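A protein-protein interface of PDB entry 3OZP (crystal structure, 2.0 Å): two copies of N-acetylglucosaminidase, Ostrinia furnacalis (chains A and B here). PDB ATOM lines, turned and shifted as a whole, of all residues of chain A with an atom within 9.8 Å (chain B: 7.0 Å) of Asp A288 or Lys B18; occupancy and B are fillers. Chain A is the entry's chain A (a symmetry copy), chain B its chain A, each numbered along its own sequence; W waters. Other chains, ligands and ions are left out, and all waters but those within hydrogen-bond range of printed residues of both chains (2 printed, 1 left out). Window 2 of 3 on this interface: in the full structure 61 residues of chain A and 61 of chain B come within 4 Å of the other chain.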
ATOM      1  N   ASN A 240     -36.444  -3.535  -0.240  1.00  0.00           N
ATOM      2  CA  ASN A 240     -35.378  -3.457   0.769  1.00  0.00           C
ATOM      3  C   ASN A 240     -34.059  -4.111   0.335  1.00  0.00           C
ATOM      4  O   ASN A 240     -32.986  -3.713   0.793  1.00  0.00           O
ATOM      5  CB  ASN A 240     -35.837  -4.038   2.112  1.00  0.00           C
ATOM      6  CG  ASN A 240     -36.630  -3.043   2.955  1.00  0.00           C
ATOM      7  OD1 ASN A 240     -37.115  -3.390   4.035  1.00  0.00           O
ATOM      8  ND2 ASN A 240     -36.761  -1.807   2.475  1.00  0.00           N
ATOM      9  N   LEU A 241     -34.138  -5.112  -0.540  1.00  0.00           N
ATOM     10  CA  LEU A 241     -32.933  -5.772  -1.045  1.00  0.00           C
ATOM     11  C   LEU A 241     -31.996  -4.792  -1.752  1.00  0.00           C
ATOM     12  O   LEU A 241     -30.799  -4.783  -1.479  1.00  0.00           O
ATOM     13  CB  LEU A 241     -33.273  -6.958  -1.956  1.00  0.00           C
ATOM     14  CG  LEU A 241     -34.025  -8.133  -1.319  1.00  0.00           C
ATOM     15  CD1 LEU A 241     -34.524  -9.057  -2.415  1.00  0.00           C
ATOM     16  CD2 LEU A 241     -33.149  -8.892  -0.319  1.00  0.00           C
ATOM     17  N   LYS A 243     -32.469  -1.324  -1.659  1.00  0.00           N
ATOM     18  CA  LYS A 243     -32.301  -0.184  -0.750  1.00  0.00           C
ATOM     19  C   LYS A 243     -31.154  -0.409   0.233  1.00  0.00           C
ATOM     20  O   LYS A 243     -30.326   0.476   0.418  1.00  0.00           O
ATOM     21  CB  LYS A 243     -33.600   0.151  -0.010  1.00  0.00           C
ATOM     22  CG  LYS A 243     -34.649   0.821  -0.889  1.00  0.00           C
ATOM     23  CD  LYS A 243     -35.831   1.325  -0.068  1.00  0.00           C
ATOM     24  CE  LYS A 243     -37.122   1.306  -0.877  1.00  0.00           C
ATOM     25  NZ  LYS A 243     -37.014   2.047  -2.171  1.00  0.00           N
ATOM     26  N   PHE A 244     -31.097  -1.591   0.846  1.00  0.00           N
ATOM     27  CA  PHE A 244     -30.003  -1.918   1.762  1.00  0.00           C
ATOM     28  C   PHE A 244     -28.765  -2.407   1.014  1.00  0.00           C
ATOM     29  O   PHE A 244     -27.645  -2.254   1.502  1.00  0.00           O
ATOM     30  CB  PHE A 244     -30.398  -2.988   2.790  1.00  0.00           C
ATOM     31  CG  PHE A 244     -31.606  -2.647   3.632  1.00  0.00           C
ATOM     32  CD1 PHE A 244     -32.070  -1.336   3.749  1.00  0.00           C
ATOM     33  CD2 PHE A 244     -32.261  -3.653   4.341  1.00  0.00           C
ATOM     34  CE1 PHE A 244     -33.187  -1.038   4.536  1.00  0.00           C
ATOM     35  CE2 PHE A 244     -33.372  -3.366   5.138  1.00  0.00           C
ATOM     36  CZ  PHE A 244     -33.835  -2.054   5.233  1.00  0.00           C
ATOM     37  N   GLY A 245     -28.979  -3.003  -0.159  1.00  0.00           N
ATOM     38  CA  GLY A 245     -27.926  -3.723  -0.870  1.00  0.00           C
ATOM     39  C   GLY A 245     -27.067  -2.926  -1.828  1.00  0.00           C
ATOM     40  O   GLY A 245     -25.928  -3.299  -2.082  1.00  0.00           O
ATOM     41  N   GLY A 283     -25.547 -11.556   0.413  1.00  0.00           N
ATOM     42  CA  GLY A 283     -25.126 -10.834   1.605  1.00  0.00           C
ATOM     43  C   GLY A 283     -25.832  -9.508   1.734  1.00  0.00           C
ATOM     44  O   GLY A 283     -26.890  -9.416   2.364  1.00  0.00           O
ATOM     45  N   GLU A 284     -25.248  -8.482   1.120  1.00  0.00           N
ATOM     46  CA  GLU A 284     -25.812  -7.136   1.156  1.00  0.00           C
ATOM     47  C   GLU A 284     -27.220  -7.110   0.579  1.00  0.00           C
ATOM     48  O   GLU A 284     -27.483  -7.681  -0.488  1.00  0.00           O
ATOM     49  CB  GLU A 284     -24.909  -6.143   0.415  1.00  0.00           C
ATOM     50  CG  GLU A 284     -23.622  -5.792   1.159  1.00  0.00           C
ATOM     51  CD  GLU A 284     -23.835  -4.859   2.357  1.00  0.00           C
ATOM     52  OE1 GLU A 284     -22.895  -4.707   3.165  1.00  0.00           O
ATOM     53  OE2 GLU A 284     -24.928  -4.270   2.490  1.00  0.00           O
ATOM     54  N   GLY A 285     -28.117  -6.441   1.299  1.00  0.00           N
ATOM     55  CA  GLY A 285     -29.517  -6.341   0.906  1.00  0.00           C
ATOM     56  C   GLY A 285     -30.422  -7.222   1.744  1.00  0.00           C
ATOM     57  O   GLY A 285     -31.602  -6.918   1.920  1.00  0.00           O
ATOM     58  N   TRP A 286     -29.861  -8.312   2.259  1.00  0.00           N
ATOM     59  CA  TRP A 286     -30.633  -9.312   2.995  1.00  0.00           C
ATOM     60  C   TRP A 286     -30.709  -9.050   4.506  1.00  0.00           C
ATOM     61  O   TRP A 286     -31.323  -9.831   5.240  1.00  0.00           O
ATOM     62  CB  TRP A 286     -30.089 -10.718   2.712  1.00  0.00           C
ATOM     63  CG  TRP A 286     -30.313 -11.156   1.293  1.00  0.00           C
ATOM     64  CD1 TRP A 286     -29.473 -10.962   0.232  1.00  0.00           C
ATOM     65  CD2 TRP A 286     -31.463 -11.838   0.774  1.00  0.00           C
ATOM     66  NE1 TRP A 286     -30.023 -11.489  -0.913  1.00  0.00           N
ATOM     67  CE2 TRP A 286     -31.245 -12.031  -0.609  1.00  0.00           C
ATOM     68  CE3 TRP A 286     -32.657 -12.306   1.343  1.00  0.00           C
ATOM     69  CZ2 TRP A 286     -32.174 -12.675  -1.431  1.00  0.00           C
ATOM     70  CZ3 TRP A 286     -33.581 -12.950   0.523  1.00  0.00           C
ATOM     71  CH2 TRP A 286     -33.333 -13.126  -0.848  1.00  0.00           C
ATOM     72  N   GLN A 287     -30.100  -7.955   4.961  1.00  0.00           N
ATOM     73  CA  GLN A 287     -30.121  -7.584   6.385  1.00  0.00           C
ATOM     74  C   GLN A 287     -31.551  -7.449   6.905  1.00  0.00           C
ATOM     75  O   GLN A 287     -32.441  -6.980   6.184  1.00  0.00           O
ATOM     76  CB  GLN A 287     -29.351  -6.278   6.645  1.00  0.00           C
ATOM     77  CG  GLN A 287     -27.832  -6.358   6.418  1.00  0.00           C
ATOM     78  CD  GLN A 287     -27.388  -5.781   5.073  1.00  0.00           C
ATOM     79  OE1 GLN A 287     -26.278  -5.259   4.948  1.00  0.00           O
ATOM     80  NE2 GLN A 287     -28.253  -5.859   4.073  1.00  0.00           N
ATOM     81  N   ASP A 288     -31.758  -7.874   8.151  1.00  0.00           N
ATOM     82  CA  ASP A 288     -33.061  -7.796   8.846  1.00  0.00           C
ATOM     83  C   ASP A 288     -34.096  -8.838   8.399  1.00  0.00           C
ATOM     84  O   ASP A 288     -35.196  -8.887   8.957  1.00  0.00           O
ATOM     85  CB  ASP A 288     -33.681  -6.387   8.769  1.00  0.00           C
ATOM     86  CG  ASP A 288     -32.753  -5.292   9.281  1.00  0.00           C
ATOM     87  OD1 ASP A 288     -31.959  -5.536  10.221  1.00  0.00           O
ATOM     88  OD2 ASP A 288     -32.834  -4.168   8.735  1.00  0.00           O
ATOM     89  N   THR A 289     -33.765  -9.655   7.401  1.00  0.00           N
ATOM     90  CA  THR A 289     -34.696 -10.684   6.925  1.00  0.00           C
ATOM     91  C   THR A 289     -34.560 -11.994   7.699  1.00  0.00           C
ATOM     92  O   THR A 289     -35.509 -12.773   7.771  1.00  0.00           O
ATOM     93  CB  THR A 289     -34.517 -11.006   5.425  1.00  0.00           C
ATOM     94  OG1 THR A 289     -33.245 -11.634   5.214  1.00  0.00           O
ATOM     95  CG2 THR A 289     -34.644  -9.750   4.566  1.00  0.00           C
ATOM     96  N   ASP A 290     -33.376 -12.229   8.262  1.00  0.00           N
ATOM     97  CA  ASP A 290     -33.021 -13.510   8.884  1.00  0.00           C
ATOM     98  C   ASP A 290     -33.016 -14.684   7.876  1.00  0.00           C
ATOM     99  O   ASP A 290     -33.136 -15.856   8.259  1.00  0.00           O
ATOM    100  CB  ASP A 290     -33.933 -13.805  10.087  1.00  0.00           C
ATOM    101  CG  ASP A 290     -33.327 -14.808  11.052  1.00  0.00           C
ATOM    102  OD1 ASP A 290     -34.067 -15.711  11.501  1.00  0.00           O
ATOM    103  OD2 ASP A 290     -32.117 -14.701  11.359  1.00  0.00           O
ATOM    104  N   LEU A 291     -32.854 -14.359   6.593  1.00  0.00           N
ATOM    105  CA  LEU A 291     -32.863 -15.361   5.523  1.00  0.00           C
ATOM    106  C   LEU A 291     -31.463 -15.761   5.039  1.00  0.00           C
ATOM    107  O   LEU A 291     -31.325 -16.617   4.164  1.00  0.00           O
ATOM    108  CB  LEU A 291     -33.724 -14.889   4.351  1.00  0.00           C
ATOM    109  CG  LEU A 291     -35.208 -14.629   4.633  1.00  0.00           C
ATOM    110  CD1 LEU A 291     -35.859 -13.986   3.434  1.00  0.00           C
ATOM    111  CD2 LEU A 291     -35.943 -15.906   5.022  1.00  0.00           C
ATOM    112  N   THR A 292     -30.435 -15.138   5.609  1.00  0.00           N
ATOM    113  CA  THR A 292     -29.056 -15.517   5.319  1.00  0.00           C
ATOM    114  C   THR A 292     -28.326 -15.961   6.577  1.00  0.00           C
ATOM    115  O   THR A 292     -28.767 -15.684   7.696  1.00  0.00           O
ATOM    116  CB  THR A 292     -28.251 -14.365   4.663  1.00  0.00           C
ATOM    117  OG1 THR A 292     -28.249 -13.220   5.525  1.00  0.00           O
ATOM    118  CG2 THR A 292     -28.837 -13.997   3.304  1.00  0.00           C
ATOM    119  N   PHE A 295     -23.238 -13.841   7.010  1.00  0.00           N
ATOM    120  CA  PHE A 295     -22.936 -12.568   6.363  1.00  0.00           C
ATOM    121  C   PHE A 295     -21.867 -11.843   7.168  1.00  0.00           C
ATOM    122  O   PHE A 295     -22.031 -11.617   8.368  1.00  0.00           O
ATOM    123  CB  PHE A 295     -24.175 -11.692   6.151  1.00  0.00           C
ATOM    124  CG  PHE A 295     -23.875 -10.369   5.486  1.00  0.00           C
ATOM    125  CD1 PHE A 295     -23.104 -10.315   4.322  1.00  0.00           C
ATOM    126  CD2 PHE A 295     -24.359  -9.178   6.020  1.00  0.00           C
ATOM    127  CE1 PHE A 295     -22.816  -9.098   3.708  1.00  0.00           C
ATOM    128  CE2 PHE A 295     -24.083  -7.955   5.405  1.00  0.00           C
ATOM    129  CZ  PHE A 295     -23.308  -7.918   4.246  1.00  0.00           C
ATOM    130  N   LYS A 296     -20.758 -11.525   6.499  1.00  0.00           N
ATOM    131  CA  LYS A 296     -19.593 -10.883   7.128  1.00  0.00           C
ATOM    132  C   LYS A 296     -18.939 -11.729   8.222  1.00  0.00           C
ATOM    133  O   LYS A 296     -18.275 -11.191   9.113  1.00  0.00           O
ATOM    134  CB  LYS A 296     -19.958  -9.496   7.666  1.00  0.00           C
ATOM    135  CG  LYS A 296     -19.982  -8.419   6.606  1.00  0.00           C
ATOM    136  CD  LYS A 296     -21.028  -7.365   6.904  1.00  0.00           C
ATOM    137  CE  LYS A 296     -20.663  -6.483   8.072  1.00  0.00           C
ATOM    138  NZ  LYS A 296     -21.790  -5.558   8.373  1.00  0.00           N
ATOM    139  N   LYS A 316     -35.720 -21.814   5.680  1.00  0.00           N
ATOM    140  CA  LYS A 316     -36.763 -20.814   5.880  1.00  0.00           C
ATOM    141  C   LYS A 316     -37.712 -20.782   4.683  1.00  0.00           C
ATOM    142  O   LYS A 316     -37.288 -20.522   3.555  1.00  0.00           O
ATOM    143  CB  LYS A 316     -36.141 -19.431   6.102  1.00  0.00           C
ATOM    144  CG  LYS A 316     -35.217 -19.334   7.311  1.00  0.00           C
ATOM    145  CD  LYS A 316     -36.007 -19.156   8.601  1.00  0.00           C
ATOM    146  CE  LYS A 316     -35.108 -19.225   9.823  1.00  0.00           C
ATOM    147  NZ  LYS A 316     -34.254 -18.017   9.955  1.00  0.00           N
ATOM    148  N   GLU A 318     -40.050 -18.663   4.014  1.00  0.00           N
ATOM    149  CA  GLU A 318     -40.190 -17.291   3.518  1.00  0.00           C
ATOM    150  C   GLU A 318     -39.180 -16.974   2.406  1.00  0.00           C
ATOM    151  O   GLU A 318     -39.473 -16.189   1.510  1.00  0.00           O
ATOM    152  CB  GLU A 318     -40.045 -16.289   4.669  1.00  0.00           C
ATOM    153  CG  GLU A 318     -40.427 -14.858   4.298  1.00  0.00           C
ATOM    154  CD  GLU A 318     -40.197 -13.861   5.429  1.00  0.00           C
ATOM    155  OE1 GLU A 318     -40.600 -12.691   5.268  1.00  0.00           O
ATOM    156  OE2 GLU A 318     -39.617 -14.238   6.472  1.00  0.00           O
ATOM    157  N   TYR A 322     -39.408 -14.709  -1.256  1.00  0.00           N
ATOM    158  CA  TYR A 322     -38.461 -13.689  -1.731  1.00  0.00           C
ATOM    159  C   TYR A 322     -37.916 -14.056  -3.117  1.00  0.00           C
ATOM    160  O   TYR A 322     -37.930 -13.238  -4.034  1.00  0.00           O
ATOM    161  CB  TYR A 322     -37.291 -13.536  -0.760  1.00  0.00           C
ATOM    162  CG  TYR A 322     -37.458 -12.481   0.309  1.00  0.00           C
ATOM    163  CD1 TYR A 322     -36.717 -11.302   0.263  1.00  0.00           C
ATOM    164  CD2 TYR A 322     -38.339 -12.669   1.377  1.00  0.00           C
ATOM    165  CE1 TYR A 322     -36.851 -10.327   1.249  1.00  0.00           C
ATOM    166  CE2 TYR A 322     -38.481 -11.705   2.373  1.00  0.00           C
ATOM    167  CZ  TYR A 322     -37.734 -10.535   2.299  1.00  0.00           C
ATOM    168  OH  TYR A 322     -37.863  -9.578   3.272  1.00  0.00           O
ATOM    169  N   VAL B   4     -28.951   4.992   3.015  1.00  0.00           N
ATOM    170  CA  VAL B   4     -29.643   4.272   4.072  1.00  0.00           C
ATOM    171  C   VAL B   4     -28.707   3.974   5.245  1.00  0.00           C
ATOM    172  O   VAL B   4     -29.152   3.617   6.338  1.00  0.00           O
ATOM    173  CB  VAL B   4     -30.271   2.972   3.466  1.00  0.00           C
ATOM    174  CG1 VAL B   4     -29.995   1.723   4.306  1.00  0.00           C
ATOM    175  CG2 VAL B   4     -31.757   3.165   3.204  1.00  0.00           C
ATOM    176  N   TRP B   5     -27.410   4.138   5.007  1.00  0.00           N
ATOM    177  CA  TRP B   5     -26.386   3.741   5.961  1.00  0.00           C
ATOM    178  C   TRP B   5     -25.697   4.932   6.618  1.00  0.00           C
ATOM    179  O   TRP B   5     -25.796   6.062   6.149  1.00  0.00           O
ATOM    180  CB  TRP B   5     -25.335   2.866   5.268  1.00  0.00           C
ATOM    181  CG  TRP B   5     -25.911   1.632   4.653  1.00  0.00           C
ATOM    182  CD1 TRP B   5     -26.198   1.428   3.334  1.00  0.00           C
ATOM    183  CD2 TRP B   5     -26.293   0.434   5.338  1.00  0.00           C
ATOM    184  NE1 TRP B   5     -26.731   0.175   3.152  1.00  0.00           N
ATOM    185  CE2 TRP B   5     -26.796  -0.461   4.365  1.00  0.00           C
ATOM    186  CE3 TRP B   5     -26.249   0.024   6.678  1.00  0.00           C
ATOM    187  CZ2 TRP B   5     -27.261  -1.739   4.691  1.00  0.00           C
ATOM    188  CZ3 TRP B   5     -26.710  -1.254   7.003  1.00  0.00           C
ATOM    189  CH2 TRP B   5     -27.212  -2.117   6.009  1.00  0.00           C
ATOM    190  N   ARG B   6     -24.999   4.651   7.711  1.00  0.00           N
ATOM    191  CA  ARG B   6     -24.099   5.604   8.339  1.00  0.00           C
ATOM    192  C   ARG B   6     -22.845   4.845   8.742  1.00  0.00           C
ATOM    193  O   ARG B   6     -22.836   3.611   8.761  1.00  0.00           O
ATOM    194  CB  ARG B   6     -24.756   6.267   9.559  1.00  0.00           C
ATOM    195  CG  ARG B   6     -25.120   5.295  10.672  1.00  0.00           C
ATOM    196  CD  ARG B   6     -25.673   6.017  11.895  1.00  0.00           C
ATOM    197  NE  ARG B   6     -25.893   5.086  12.997  1.00  0.00           N
ATOM    198  CZ  ARG B   6     -24.979   4.768  13.912  1.00  0.00           C
ATOM    199  NH1 ARG B   6     -23.763   5.305  13.874  1.00  0.00           N
ATOM    200  NH2 ARG B   6     -25.284   3.912  14.875  1.00  0.00           N
ATOM    201  N   VAL B  15     -17.017   1.557  10.321  1.00  0.00           N
ATOM    202  CA  VAL B  15     -17.935   0.427  10.179  1.00  0.00           C
ATOM    203  C   VAL B  15     -19.322   0.881   9.757  1.00  0.00           C
ATOM    204  O   VAL B  15     -19.850   1.872  10.270  1.00  0.00           O
ATOM    205  CB  VAL B  15     -17.945  -0.556  11.412  1.00  0.00           C
ATOM    206  CG1 VAL B  15     -16.659  -0.439  12.232  1.00  0.00           C
ATOM    207  CG2 VAL B  15     -19.166  -0.374  12.289  1.00  0.00           C
ATOM    208  N   LYS B  16     -19.888   0.169   8.790  1.00  0.00           N
ATOM    209  CA  LYS B  16     -21.185   0.517   8.241  1.00  0.00           C
ATOM    210  C   LYS B  16     -22.288   0.060   9.184  1.00  0.00           C
ATOM    211  O   LYS B  16     -22.340  -1.104   9.587  1.00  0.00           O
ATOM    212  CB  LYS B  16     -21.377  -0.098   6.853  1.00  0.00           C
ATOM    213  CG  LYS B  16     -22.543   0.503   6.082  1.00  0.00           C
ATOM    214  CD  LYS B  16     -22.657  -0.039   4.666  1.00  0.00           C
ATOM    215  CE  LYS B  16     -23.324  -1.413   4.632  1.00  0.00           C
ATOM    216  NZ  LYS B  16     -23.811  -1.725   3.258  1.00  0.00           N
ATOM    217  N   LEU B  17     -23.161   0.996   9.533  1.00  0.00           N
ATOM    218  CA  LEU B  17     -24.261   0.726  10.442  1.00  0.00           C
ATOM    219  C   LEU B  17     -25.539   1.292   9.864  1.00  0.00           C
ATOM    220  O   LEU B  17     -25.510   2.285   9.135  1.00  0.00           O
ATOM    221  CB  LEU B  17     -23.982   1.336  11.826  1.00  0.00           C
ATOM    222  CG  LEU B  17     -22.798   0.780  12.627  1.00  0.00           C
ATOM    223  CD1 LEU B  17     -22.482   1.662  13.829  1.00  0.00           C
ATOM    224  CD2 LEU B  17     -23.034  -0.664  13.064  1.00  0.00           C
ATOM    225  N   LYS B  18     -26.662   0.652  10.175  1.00  0.00           N
ATOM    226  CA  LYS B  18     -27.957   1.168   9.755  1.00  0.00           C
ATOM    227  C   LYS B  18     -28.165   2.552  10.357  1.00  0.00           C
ATOM    228  O   LYS B  18     -27.878   2.768  11.539  1.00  0.00           O
ATOM    229  CB  LYS B  18     -29.082   0.232  10.200  1.00  0.00           C
ATOM    230  CG  LYS B  18     -30.341   0.330   9.357  1.00  0.00           C
ATOM    231  CD  LYS B  18     -30.050  -0.027   7.901  1.00  0.00           C
ATOM    232  CE  LYS B  18     -31.116  -0.940   7.329  1.00  0.00           C
ATOM    233  NZ  LYS B  18     -31.004  -2.336   7.852  1.00  0.00           N
ATOM    234  N   ASN B  19     -28.628   3.491   9.539  1.00  0.00           N
ATOM    235  CA  ASN B  19     -28.980   4.816  10.033  1.00  0.00           C
ATOM    236  C   ASN B  19     -30.409   4.772  10.572  1.00  0.00           C
ATOM    237  O   ASN B  19     -31.353   5.191   9.903  1.00  0.00           O
ATOM    238  CB  ASN B  19     -28.817   5.874   8.931  1.00  0.00           C
ATOM    239  CG  ASN B  19     -29.017   7.305   9.439  1.00  0.00           C
ATOM    240  OD1 ASN B  19     -29.312   8.210   8.658  1.00  0.00           O
ATOM    241  ND2 ASN B  19     -28.847   7.511  10.742  1.00  0.00           N
ATOM    242  N   ASP B  20     -30.554   4.224  11.774  1.00  0.00           N
ATOM    243  CA  ASP B  20     -31.865   4.042  12.401  1.00  0.00           C
ATOM    244  C   ASP B  20     -32.396   5.375  12.937  1.00  0.00           C
ATOM    245  O   ASP B  20     -31.642   6.126  13.558  1.00  0.00           O
ATOM    246  CB  ASP B  20     -31.791   2.991  13.513  1.00  0.00           C
ATOM    247  CG  ASP B  20     -31.709   1.561  12.969  1.00  0.00           C
ATOM    248  OD1 ASP B  20     -31.048   0.721  13.614  1.00  0.00           O
ATOM    249  OD2 ASP B  20     -32.306   1.271  11.905  1.00  0.00           O
ATOM    250  N   PRO B  21     -33.687   5.673  12.680  1.00  0.00           N
ATOM    251  CA  PRO B  21     -34.302   6.966  13.014  1.00  0.00           C
ATOM    252  C   PRO B  21     -34.386   7.278  14.517  1.00  0.00           C
ATOM    253  O   PRO B  21     -34.405   8.454  14.894  1.00  0.00           O
ATOM    254  CB  PRO B  21     -35.711   6.851  12.416  1.00  0.00           C
ATOM    255  CG  PRO B  21     -35.965   5.382  12.307  1.00  0.00           C
ATOM    256  CD  PRO B  21     -34.632   4.794  11.965  1.00  0.00           C
HETATM  257  O   HOH W   1     -20.599  -3.277   9.389  1.00  0.00           O
HETATM  258  O   HOH W   2     -27.622   0.877   0.326  1.00  0.00           O
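The side-chain amino group (NZ) of Lys B18 lies within salt-bridge range of the side-chain carboxylate (OD2) of Asp A288 (2.7 Å).
OE2 of Glu A284 lies within salt-bridge range of NZ of Lys B16 (2.9 Å).
The indole nitrogen (NE1) of Trp B5 sits at hydrogen-bond distance from the backbone carbonyl oxygen (O) of Phe A244, 3.1 Å away.
The side-chain amide nitrogen (NE2) of Gln A287 sits close to the backbone NH (N) of Gly A285, 2.8 Å away.
The backbone carbonyl oxygen (O) of Lys B18 sits at hydrogen-bond distance from the guanidinium group (NE) of Arg B6 (3.4 Å).
The backbone carbonyl oxygen (O) of Val B4 sits at hydrogen-bond distance from the backbone NH (N) of Asn B19 (3.2 Å).
The side-chain amide oxygen (OE1) of Gln A287 lies close to the side-chain carboxylate (OE2) of Glu A284, at 3.0 Å.
Lys A243 touches Val B4.
CD1 of Phe A244 touches CG1 of Val B4, at 3.7 Å.
Lys B18 touches Phe A244 (CE to CE1, 3.5 Å).
OE1 of Gln A287 touches CH2 of Trp B5, at 3.4 Å.
Of the printed residues of chain B, Phe A244 touches Val B4, Trp B5 and Lys B18.
Gly A245 touches none of the printed residues of chain B.
Printed residues of chain A within 4 Å of Val B4: Lys A243 and Phe A244.
Printed residues of chain A within 4 Å of Trp B5: Phe A244 and Gln A287.
No residue of chain A comes within 4 Å of Leu B17.
Lys B18 touches two residues of chain A.
No residue of chain A comes within 4 Å of Asp B20.
The nearest residue of chain A that does not touch Lys B18 is Gln A287 (4.4 Å).
Of the 10 printed residues of chain B, 4 touch a printed residue of chain A.
Printed residues of chain B that touch a printed residue of chain A: Val B4, Trp B5, Lys B16 and Lys B18.
Of the 20 printed residues of chain A, 5 touch a printed residue of chain B.
Hydrophobic or aromatic side chains of chain A within 4 Å of the printed part of chain B: Phe A244.
Along chain A the printed residues that touch a printed residue of chain B span positions 243 to 288.
Among the printed residues, 7 pairs touch across the chains.
Among the printed residues, Asp or Glu carboxylates within 4 Å of a Lys or Arg side-chain nitrogen of the other chain: Glu A284 with Lys B16 and Asp A288 with Lys B18.
No position is printed for both chains.
Water W2 lies within hydrogen-bond range of the backbone carbonyl oxygen of Lys A243 (2.7 Å), the indole nitrogen of Trp B5 (3.0 Å) and the backbone carbonyl oxygen of Phe A244 (3.3 Å).
Water W1 lies within hydrogen-bond range of the side-chain amino group (NZ) of Lys A296 (2.8 Å) and the backbone carbonyl oxygen (O) of Lys B16 (2.8 Å).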
